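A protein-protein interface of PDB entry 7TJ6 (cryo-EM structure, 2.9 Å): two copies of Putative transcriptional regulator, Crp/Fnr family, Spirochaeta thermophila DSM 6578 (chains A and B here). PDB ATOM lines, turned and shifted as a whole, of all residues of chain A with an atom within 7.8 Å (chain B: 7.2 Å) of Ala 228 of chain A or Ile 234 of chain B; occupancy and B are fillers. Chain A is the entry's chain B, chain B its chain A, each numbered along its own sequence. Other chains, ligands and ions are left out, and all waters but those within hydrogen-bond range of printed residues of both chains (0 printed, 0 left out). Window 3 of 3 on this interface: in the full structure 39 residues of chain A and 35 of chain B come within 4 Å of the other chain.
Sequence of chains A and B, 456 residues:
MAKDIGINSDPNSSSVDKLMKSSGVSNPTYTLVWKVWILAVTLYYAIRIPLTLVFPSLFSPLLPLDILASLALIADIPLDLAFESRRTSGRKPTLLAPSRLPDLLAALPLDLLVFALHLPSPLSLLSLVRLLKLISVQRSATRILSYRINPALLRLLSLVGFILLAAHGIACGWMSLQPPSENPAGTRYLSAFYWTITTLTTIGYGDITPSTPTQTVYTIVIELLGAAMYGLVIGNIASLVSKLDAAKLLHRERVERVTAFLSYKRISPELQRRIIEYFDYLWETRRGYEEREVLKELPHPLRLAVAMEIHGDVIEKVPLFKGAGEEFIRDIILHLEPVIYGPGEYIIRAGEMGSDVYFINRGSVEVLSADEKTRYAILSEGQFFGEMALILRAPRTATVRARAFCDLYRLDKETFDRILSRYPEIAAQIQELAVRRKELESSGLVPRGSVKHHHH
O of Leu 224 of chain A sits at hydrogen-bond distance from OH of Tyr 230 of chain B, at 3.4 Å.
Among the printed residues, pairs that only touch across the chains: Glu 223 of chain A with Ile 203 of chain B (3.4 Å), Glu 223 of chain A with Thr 201 of chain B (3.5 Å), Thr 202 of chain A with Ile 203 of chain B (3.7 Å), Thr 199 of chain A with Ile 203 of chain B (3.7 Å), Ala 228 of chain A with Ile 234 of chain B (3.8 Å) and Leu 232 of chain A with Ala 238 of chain B (3.9 Å).
Ala 228 of chain A touches one residue of chain B.
Of chain A, only Ala 228 comes within 4 Å of Ile 234 of chain B.
Ala 227 of chain A touches none of the printed residues of chain B.
No residue of chain A comes within 4 Å of Gly 235 of chain B.
Of the printed residues of chain B, Leu 232 of chain A touches Ala 238.
Printed residues of chain A within 4 Å of Ile 203 of chain B: Thr 199 (3.7 Å), Thr 202 (3.7 Å) and Glu 223 (3.4 Å).
Of the printed residues of chain B, Glu 223 of chain A touches Thr 201 (3.5 Å) and Ile 203 (3.4 Å).
Printed residues of chain A within 4 Å of Ala 238 of chain B: Leu 232.
The nearest residue of chain A that does not touch Ile 234 of chain B is Leu 232 of chain A (5.6 Å).
Along chain A the printed residues that touch a printed residue of chain B span positions 199 to 232.
Of the 17 printed residues of chain B, 5 touch a printed residue of chain A.
Hydrophobic or aromatic side chains of chain B within 4 Å of the printed part of chain A: Ile 203, Tyr 230, Ile 234 and Ala 238.
Along chain B the printed residues that touch a printed residue of chain A span positions 201 to 238.
Among the printed residues, no Asp or Glu carboxylate lies within 4 Å of a Lys or Arg side-chain nitrogen of the other chain.
Ala 228 of chain A touches Ile 234 of chain B, but with the chains exchanged Ile 234 of chain A does not touch Ala 228 of chain B (16.6 Å).
Positions printed for both chains: 228, 229, 230, 231, 232, 233, 234 and 235.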
ATOM      1  N   THR A 199     -27.474  21.668  23.157  1.00  0.00           N
ATOM      2  CA  THR A 199     -26.042  21.514  22.941  1.00  0.00           C
ATOM      3  C   THR A 199     -25.723  21.205  21.480  1.00  0.00           C
ATOM      4  O   THR A 199     -24.835  21.828  20.892  1.00  0.00           O
ATOM      5  CB  THR A 199     -25.484  20.430  23.854  1.00  0.00           C
ATOM      6  OG1 THR A 199     -25.767  20.773  25.214  1.00  0.00           O
ATOM      7  CG2 THR A 199     -23.987  20.346  23.690  1.00  0.00           C
ATOM      8  N   LEU A 200     -26.426  20.234  20.874  1.00  0.00           N
ATOM      9  CA  LEU A 200     -26.101  19.842  19.503  1.00  0.00           C
ATOM     10  C   LEU A 200     -26.339  20.957  18.498  1.00  0.00           C
ATOM     11  O   LEU A 200     -25.679  20.987  17.457  1.00  0.00           O
ATOM     12  CB  LEU A 200     -26.899  18.618  19.057  1.00  0.00           C
ATOM     13  CG  LEU A 200     -26.617  17.215  19.580  1.00  0.00           C
ATOM     14  CD1 LEU A 200     -27.893  16.422  19.509  1.00  0.00           C
ATOM     15  CD2 LEU A 200     -25.548  16.544  18.773  1.00  0.00           C
ATOM     16  N   THR A 202     -25.758  24.141  19.003  1.00  0.00           N
ATOM     17  CA  THR A 202     -24.881  25.257  19.355  1.00  0.00           C
ATOM     18  C   THR A 202     -25.673  26.516  19.688  1.00  0.00           C
ATOM     19  O   THR A 202     -25.295  27.626  19.314  1.00  0.00           O
ATOM     20  CB  THR A 202     -23.848  25.537  18.261  1.00  0.00           C
ATOM     21  OG1 THR A 202     -24.473  26.233  17.179  1.00  0.00           O
ATOM     22  CG2 THR A 202     -23.226  24.247  17.756  1.00  0.00           C
ATOM     23  N   VAL A 221     -17.344  16.365  25.879  1.00  0.00           N
ATOM     24  CA  VAL A 221     -17.290  15.430  24.763  1.00  0.00           C
ATOM     25  C   VAL A 221     -18.437  15.686  23.804  1.00  0.00           C
ATOM     26  O   VAL A 221     -18.256  15.678  22.579  1.00  0.00           O
ATOM     27  CB  VAL A 221     -17.276  13.988  25.285  1.00  0.00           C
ATOM     28  CG1 VAL A 221     -17.455  13.048  24.141  1.00  0.00           C
ATOM     29  CG2 VAL A 221     -15.964  13.729  26.023  1.00  0.00           C
ATOM     30  N   ILE A 222     -19.631  15.931  24.343  1.00  0.00           N
ATOM     31  CA  ILE A 222     -20.788  16.203  23.494  1.00  0.00           C
ATOM     32  C   ILE A 222     -20.558  17.475  22.686  1.00  0.00           C
ATOM     33  O   ILE A 222     -20.772  17.496  21.472  1.00  0.00           O
ATOM     34  CB  ILE A 222     -22.069  16.292  24.340  1.00  0.00           C
ATOM     35  CG1 ILE A 222     -22.439  14.929  24.918  1.00  0.00           C
ATOM     36  CG2 ILE A 222     -23.223  16.792  23.497  1.00  0.00           C
ATOM     37  CD1 ILE A 222     -22.342  13.780  23.956  1.00  0.00           C
ATOM     38  N   GLU A 223     -20.088  18.543  23.339  1.00  0.00           N
ATOM     39  CA  GLU A 223     -19.846  19.796  22.627  1.00  0.00           C
ATOM     40  C   GLU A 223     -18.791  19.628  21.541  1.00  0.00           C
ATOM     41  O   GLU A 223     -18.881  20.252  20.477  1.00  0.00           O
ATOM     42  CB  GLU A 223     -19.385  20.885  23.597  1.00  0.00           C
ATOM     43  CG  GLU A 223     -20.422  21.469  24.521  1.00  0.00           C
ATOM     44  CD  GLU A 223     -19.804  22.046  25.774  1.00  0.00           C
ATOM     45  OE1 GLU A 223     -18.582  21.897  25.968  1.00  0.00           O
ATOM     46  OE2 GLU A 223     -20.528  22.692  26.549  1.00  0.00           O
ATOM     47  N   LEU A 224     -17.785  18.788  21.789  1.00  0.00           N
ATOM     48  CA  LEU A 224     -16.730  18.599  20.802  1.00  0.00           C
ATOM     49  C   LEU A 224     -17.198  17.778  19.613  1.00  0.00           C
ATOM     50  O   LEU A 224     -16.937  18.144  18.463  1.00  0.00           O
ATOM     51  CB  LEU A 224     -15.524  17.926  21.451  1.00  0.00           C
ATOM     52  CG  LEU A 224     -14.473  18.857  22.037  1.00  0.00           C
ATOM     53  CD1 LEU A 224     -13.347  18.067  22.657  1.00  0.00           C
ATOM     54  CD2 LEU A 224     -13.951  19.784  20.961  1.00  0.00           C
ATOM     55  N   LEU A 225     -17.928  16.694  19.862  1.00  0.00           N
ATOM     56  CA  LEU A 225     -18.275  15.735  18.818  1.00  0.00           C
ATOM     57  C   LEU A 225     -19.639  16.019  18.205  1.00  0.00           C
ATOM     58  O   LEU A 225     -19.750  16.145  16.982  1.00  0.00           O
ATOM     59  CB  LEU A 225     -18.205  14.297  19.352  1.00  0.00           C
ATOM     60  CG  LEU A 225     -16.821  13.638  19.465  1.00  0.00           C
ATOM     61  CD1 LEU A 225     -16.215  13.502  18.075  1.00  0.00           C
ATOM     62  CD2 LEU A 225     -15.848  14.334  20.408  1.00  0.00           C
ATOM     63  N   GLY A 226     -20.689  16.029  19.023  1.00  0.00           N
ATOM     64  CA  GLY A 226     -22.023  16.075  18.469  1.00  0.00           C
ATOM     65  C   GLY A 226     -22.301  17.383  17.760  1.00  0.00           C
ATOM     66  O   GLY A 226     -22.983  17.404  16.735  1.00  0.00           O
ATOM     67  N   ALA A 227     -21.761  18.484  18.276  1.00  0.00           N
ATOM     68  CA  ALA A 227     -21.956  19.770  17.621  1.00  0.00           C
ATOM     69  C   ALA A 227     -21.321  19.778  16.235  1.00  0.00           C
ATOM     70  O   ALA A 227     -21.945  20.199  15.254  1.00  0.00           O
ATOM     71  CB  ALA A 227     -21.384  20.889  18.488  1.00  0.00           C
ATOM     72  N   ALA A 228     -20.067  19.317  16.141  1.00  0.00           N
ATOM     73  CA  ALA A 228     -19.392  19.239  14.849  1.00  0.00           C
ATOM     74  C   ALA A 228     -20.080  18.274  13.889  1.00  0.00           C
ATOM     75  O   ALA A 228     -20.223  18.581  12.698  1.00  0.00           O
ATOM     76  CB  ALA A 228     -17.936  18.830  15.050  1.00  0.00           C
ATOM     77  N   MET A 229     -20.493  17.098  14.371  1.00  0.00           N
ATOM     78  CA  MET A 229     -21.173  16.155  13.484  1.00  0.00           C
ATOM     79  C   MET A 229     -22.479  16.750  12.986  1.00  0.00           C
ATOM     80  O   MET A 229     -22.839  16.581  11.818  1.00  0.00           O
ATOM     81  CB  MET A 229     -21.400  14.778  14.117  1.00  0.00           C
ATOM     82  CG  MET A 229     -22.340  14.675  15.284  1.00  0.00           C
ATOM     83  SD  MET A 229     -22.398  12.968  15.870  1.00  0.00           S
ATOM     84  CE  MET A 229     -23.543  13.085  17.239  1.00  0.00           C
ATOM     85  N   TYR A 230     -23.217  17.427  13.871  1.00  0.00           N
ATOM     86  CA  TYR A 230     -24.468  18.058  13.477  1.00  0.00           C
ATOM     87  C   TYR A 230     -24.226  19.128  12.432  1.00  0.00           C
ATOM     88  O   TYR A 230     -24.975  19.222  11.457  1.00  0.00           O
ATOM     89  CB  TYR A 230     -25.142  18.679  14.697  1.00  0.00           C
ATOM     90  CG  TYR A 230     -26.528  19.221  14.443  1.00  0.00           C
ATOM     91  CD1 TYR A 230     -27.522  18.410  13.940  1.00  0.00           C
ATOM     92  CD2 TYR A 230     -26.843  20.542  14.721  1.00  0.00           C
ATOM     93  CE1 TYR A 230     -28.795  18.888  13.721  1.00  0.00           C
ATOM     94  CE2 TYR A 230     -28.111  21.032  14.502  1.00  0.00           C
ATOM     95  CZ  TYR A 230     -29.082  20.202  14.004  1.00  0.00           C
ATOM     96  OH  TYR A 230     -30.345  20.697  13.788  1.00  0.00           O
ATOM     97  N   GLY A 231     -23.189  19.943  12.618  1.00  0.00           N
ATOM     98  CA  GLY A 231     -22.868  20.943  11.614  1.00  0.00           C
ATOM     99  C   GLY A 231     -22.540  20.316  10.272  1.00  0.00           C
ATOM    100  O   GLY A 231     -22.993  20.788   9.224  1.00  0.00           O
ATOM    101  N   LEU A 232     -21.764  19.229  10.288  1.00  0.00           N
ATOM    102  CA  LEU A 232     -21.401  18.560   9.043  1.00  0.00           C
ATOM    103  C   LEU A 232     -22.619  17.942   8.363  1.00  0.00           C
ATOM    104  O   LEU A 232     -22.756  18.017   7.135  1.00  0.00           O
ATOM    105  CB  LEU A 232     -20.354  17.487   9.351  1.00  0.00           C
ATOM    106  CG  LEU A 232     -19.615  16.687   8.282  1.00  0.00           C
ATOM    107  CD1 LEU A 232     -18.280  16.233   8.838  1.00  0.00           C
ATOM    108  CD2 LEU A 232     -20.424  15.474   7.874  1.00  0.00           C
ATOM    109  N   VAL A 233     -23.526  17.352   9.143  1.00  0.00           N
ATOM    110  CA  VAL A 233     -24.731  16.761   8.568  1.00  0.00           C
ATOM    111  C   VAL A 233     -25.646  17.843   8.011  1.00  0.00           C
ATOM    112  O   VAL A 233     -26.286  17.654   6.972  1.00  0.00           O
ATOM    113  CB  VAL A 233     -25.441  15.869   9.603  1.00  0.00           C
ATOM    114  CG1 VAL A 233     -26.767  15.370   9.065  1.00  0.00           C
ATOM    115  CG2 VAL A 233     -24.566  14.678   9.949  1.00  0.00           C
ATOM    116  N   ILE A 234     -25.727  18.991   8.687  1.00  0.00           N
ATOM    117  CA  ILE A 234     -26.512  20.106   8.166  1.00  0.00           C
ATOM    118  C   ILE A 234     -25.930  20.603   6.849  1.00  0.00           C
ATOM    119  O   ILE A 234     -26.668  20.923   5.911  1.00  0.00           O
ATOM    120  CB  ILE A 234     -26.627  21.233   9.211  1.00  0.00           C
ATOM    121  CG1 ILE A 234     -27.434  20.755  10.417  1.00  0.00           C
ATOM    122  CG2 ILE A 234     -27.267  22.473   8.614  1.00  0.00           C
ATOM    123  CD1 ILE A 234     -28.878  20.451  10.099  1.00  0.00           C
ATOM    124  N   GLY A 235     -24.601  20.699   6.765  1.00  0.00           N
ATOM    125  CA  GLY A 235     -23.988  21.070   5.497  1.00  0.00           C
ATOM    126  C   GLY A 235     -24.288  20.082   4.383  1.00  0.00           C
ATOM    127  O   GLY A 235     -24.586  20.479   3.249  1.00  0.00           O
ATOM    128  N   LEU B 159      -5.565  17.509  11.335  1.00  0.00           N
ATOM    129  CA  LEU B 159      -6.452  18.599  11.731  1.00  0.00           C
ATOM    130  C   LEU B 159      -7.048  18.363  13.116  1.00  0.00           C
ATOM    131  O   LEU B 159      -7.132  19.293  13.939  1.00  0.00           O
ATOM    132  CB  LEU B 159      -7.562  18.750  10.690  1.00  0.00           C
ATOM    133  CG  LEU B 159      -7.143  19.309   9.328  1.00  0.00           C
ATOM    134  CD1 LEU B 159      -8.294  19.264   8.336  1.00  0.00           C
ATOM    135  CD2 LEU B 159      -6.619  20.725   9.475  1.00  0.00           C
ATOM    136  N   ILE B 163      -6.395  20.887  16.421  1.00  0.00           N
ATOM    137  CA  ILE B 163      -7.430  21.577  17.187  1.00  0.00           C
ATOM    138  C   ILE B 163      -7.442  21.120  18.645  1.00  0.00           C
ATOM    139  O   ILE B 163      -7.658  21.929  19.556  1.00  0.00           O
ATOM    140  CB  ILE B 163      -8.809  21.433  16.513  1.00  0.00           C
ATOM    141  CG1 ILE B 163      -9.785  22.411  17.158  1.00  0.00           C
ATOM    142  CG2 ILE B 163      -9.339  20.012  16.575  1.00  0.00           C
ATOM    143  CD1 ILE B 163      -9.380  23.855  17.000  1.00  0.00           C
ATOM    144  N   THR B 201     -16.533  26.103  20.539  1.00  0.00           N
ATOM    145  CA  THR B 201     -17.561  25.468  19.724  1.00  0.00           C
ATOM    146  C   THR B 201     -18.744  26.386  19.468  1.00  0.00           C
ATOM    147  O   THR B 201     -19.707  25.966  18.821  1.00  0.00           O
ATOM    148  CB  THR B 201     -18.052  24.175  20.379  1.00  0.00           C
ATOM    149  OG1 THR B 201     -18.456  24.447  21.725  1.00  0.00           O
ATOM    150  CG2 THR B 201     -16.964  23.122  20.381  1.00  0.00           C
ATOM    151  N   ILE B 203     -20.980  27.464  21.537  1.00  0.00           N
ATOM    152  CA  ILE B 203     -22.161  27.006  22.248  1.00  0.00           C
ATOM    153  C   ILE B 203     -22.494  27.932  23.407  1.00  0.00           C
ATOM    154  O   ILE B 203     -23.659  28.263  23.624  1.00  0.00           O
ATOM    155  CB  ILE B 203     -21.975  25.545  22.710  1.00  0.00           C
ATOM    156  CG1 ILE B 203     -21.921  24.635  21.488  1.00  0.00           C
ATOM    157  CG2 ILE B 203     -23.089  25.113  23.618  1.00  0.00           C
ATOM    158  CD1 ILE B 203     -21.507  23.239  21.768  1.00  0.00           C
ATOM    159  N   ALA B 228     -13.382  31.198  15.144  1.00  0.00           N
ATOM    160  CA  ALA B 228     -13.219  31.222  13.693  1.00  0.00           C
ATOM    161  C   ALA B 228     -12.278  30.132  13.194  1.00  0.00           C
ATOM    162  O   ALA B 228     -12.558  29.487  12.176  1.00  0.00           O
ATOM    163  CB  ALA B 228     -12.715  32.592  13.251  1.00  0.00           C
ATOM    164  N   MET B 229     -11.147  29.919  13.877  1.00  0.00           N
ATOM    165  CA  MET B 229     -10.228  28.869  13.438  1.00  0.00           C
ATOM    166  C   MET B 229     -10.899  27.509  13.538  1.00  0.00           C
ATOM    167  O   MET B 229     -10.721  26.658  12.663  1.00  0.00           O
ATOM    168  CB  MET B 229      -8.890  28.880  14.184  1.00  0.00           C
ATOM    169  CG  MET B 229      -8.887  28.556  15.650  1.00  0.00           C
ATOM    170  SD  MET B 229      -7.206  28.681  16.298  1.00  0.00           S
ATOM    171  CE  MET B 229      -7.444  28.274  18.024  1.00  0.00           C
ATOM    172  N   TYR B 230     -11.650  27.277  14.617  1.00  0.00           N
ATOM    173  CA  TYR B 230     -12.355  26.015  14.784  1.00  0.00           C
ATOM    174  C   TYR B 230     -13.376  25.818  13.681  1.00  0.00           C
ATOM    175  O   TYR B 230     -13.493  24.719  13.136  1.00  0.00           O
ATOM    176  CB  TYR B 230     -13.057  25.988  16.139  1.00  0.00           C
ATOM    177  CG  TYR B 230     -13.688  24.663  16.494  1.00  0.00           C
ATOM    178  CD1 TYR B 230     -12.934  23.511  16.532  1.00  0.00           C
ATOM    179  CD2 TYR B 230     -15.035  24.571  16.808  1.00  0.00           C
ATOM    180  CE1 TYR B 230     -13.492  22.299  16.873  1.00  0.00           C
ATOM    181  CE2 TYR B 230     -15.606  23.365  17.146  1.00  0.00           C
ATOM    182  CZ  TYR B 230     -14.831  22.233  17.178  1.00  0.00           C
ATOM    183  OH  TYR B 230     -15.406  21.034  17.517  1.00  0.00           O
ATOM    184  N   GLY B 231     -14.122  26.868  13.341  1.00  0.00           N
ATOM    185  CA  GLY B 231     -15.066  26.757  12.243  1.00  0.00           C
ATOM    186  C   GLY B 231     -14.378  26.421  10.933  1.00  0.00           C
ATOM    187  O   GLY B 231     -14.850  25.572  10.169  1.00  0.00           O
ATOM    188  N   LEU B 232     -13.241  27.067  10.666  1.00  0.00           N
ATOM    189  CA  LEU B 232     -12.512  26.803   9.430  1.00  0.00           C
ATOM    190  C   LEU B 232     -11.961  25.381   9.396  1.00  0.00           C
ATOM    191  O   LEU B 232     -12.010  24.714   8.354  1.00  0.00           O
ATOM    192  CB  LEU B 232     -11.379  27.823   9.302  1.00  0.00           C
ATOM    193  CG  LEU B 232     -10.498  27.968   8.064  1.00  0.00           C
ATOM    194  CD1 LEU B 232      -9.968  29.385   7.995  1.00  0.00           C
ATOM    195  CD2 LEU B 232      -9.332  27.002   8.127  1.00  0.00           C
ATOM    196  N   VAL B 233     -11.460  24.889  10.529  1.00  0.00           N
ATOM    197  CA  VAL B 233     -10.937  23.526  10.584  1.00  0.00           C
ATOM    198  C   VAL B 233     -12.063  22.513  10.430  1.00  0.00           C
ATOM    199  O   VAL B 233     -11.890  21.469   9.793  1.00  0.00           O
ATOM    200  CB  VAL B 233     -10.127  23.310  11.876  1.00  0.00           C
ATOM    201  CG1 VAL B 233      -9.707  21.859  12.011  1.00  0.00           C
ATOM    202  CG2 VAL B 233      -8.889  24.187  11.865  1.00  0.00           C
ATOM    203  N   ILE B 234     -13.234  22.799  11.005  1.00  0.00           N
ATOM    204  CA  ILE B 234     -14.386  21.920  10.822  1.00  0.00           C
ATOM    205  C   ILE B 234     -14.802  21.879   9.358  1.00  0.00           C
ATOM    206  O   ILE B 234     -15.145  20.816   8.827  1.00  0.00           O
ATOM    207  CB  ILE B 234     -15.547  22.340  11.743  1.00  0.00           C
ATOM    208  CG1 ILE B 234     -15.163  22.133  13.207  1.00  0.00           C
ATOM    209  CG2 ILE B 234     -16.811  21.563  11.423  1.00  0.00           C
ATOM    210  CD1 ILE B 234     -14.951  20.686  13.581  1.00  0.00           C
ATOM    211  N   GLY B 235     -14.803  23.033   8.688  1.00  0.00           N
ATOM    212  CA  GLY B 235     -15.093  23.033   7.261  1.00  0.00           C
ATOM    213  C   GLY B 235     -14.096  22.219   6.454  1.00  0.00           C
ATOM    214  O   GLY B 235     -14.479  21.467   5.548  1.00  0.00           O
ATOM    215  N   ASN B 236     -12.804  22.342   6.777  1.00  0.00           N
ATOM    216  CA  ASN B 236     -11.803  21.546   6.072  1.00  0.00           C
ATOM    217  C   ASN B 236     -11.983  20.058   6.340  1.00  0.00           C
ATOM    218  O   ASN B 236     -11.820  19.233   5.434  1.00  0.00           O
ATOM    219  CB  ASN B 236     -10.392  21.975   6.468  1.00  0.00           C
ATOM    220  CG  ASN B 236     -10.066  23.380   6.037  1.00  0.00           C
ATOM    221  OD1 ASN B 236     -10.739  23.950   5.179  1.00  0.00           O
ATOM    222  ND2 ASN B 236      -9.018  23.948   6.618  1.00  0.00           N
ATOM    223  N   ILE B 237     -12.316  19.696   7.580  1.00  0.00           N
ATOM    224  CA  ILE B 237     -12.564  18.295   7.913  1.00  0.00           C
ATOM    225  C   ILE B 237     -13.780  17.756   7.168  1.00  0.00           C
ATOM    226  O   ILE B 237     -13.763  16.623   6.677  1.00  0.00           O
ATOM    227  CB  ILE B 237     -12.708  18.128   9.438  1.00  0.00           C
ATOM    228  CG1 ILE B 237     -11.350  18.313  10.121  1.00  0.00           C
ATOM    229  CG2 ILE B 237     -13.297  16.769   9.788  1.00  0.00           C
ATOM    230  CD1 ILE B 237     -11.364  18.014  11.606  1.00  0.00           C
ATOM    231  N   ALA B 238     -14.849  18.552   7.065  1.00  0.00           N
ATOM    232  CA  ALA B 238     -16.011  18.130   6.285  1.00  0.00           C
ATOM    233  C   ALA B 238     -15.654  17.901   4.821  1.00  0.00           C
ATOM    234  O   ALA B 238     -16.020  16.874   4.226  1.00  0.00           O
ATOM    235  CB  ALA B 238     -17.124  19.170   6.410  1.00  0.00           C
ATOM    236  N   SER B 239     -14.905  18.839   4.230  1.00  0.00           N
ATOM    237  CA  SER B 239     -14.502  18.684   2.835  1.00  0.00           C
ATOM    238  C   SER B 239     -13.642  17.444   2.648  1.00  0.00           C
ATOM    239  O   SER B 239     -13.821  16.693   1.685  1.00  0.00           O
ATOM    240  CB  SER B 239     -13.754  19.928   2.357  1.00  0.00           C
ATOM    241  OG  SER B 239     -14.589  21.071   2.392  1.00  0.00           O
ATOM    242  N   LEU B 240     -12.739  17.191   3.593  1.00  0.00           N
ATOM    243  CA  LEU B 240     -11.877  16.017   3.543  1.00  0.00           C
ATOM    244  C   LEU B 240     -12.669  14.723   3.694  1.00  0.00           C
ATOM    245  O   LEU B 240     -12.325  13.708   3.077  1.00  0.00           O
ATOM    246  CB  LEU B 240     -10.809  16.155   4.613  1.00  0.00           C
ATOM    247  CG  LEU B 240      -9.472  15.497   4.372  1.00  0.00           C
ATOM    248  CD1 LEU B 240      -8.816  16.093   3.153  1.00  0.00           C
ATOM    249  CD2 LEU B 240      -8.700  15.891   5.569  1.00  0.00           C
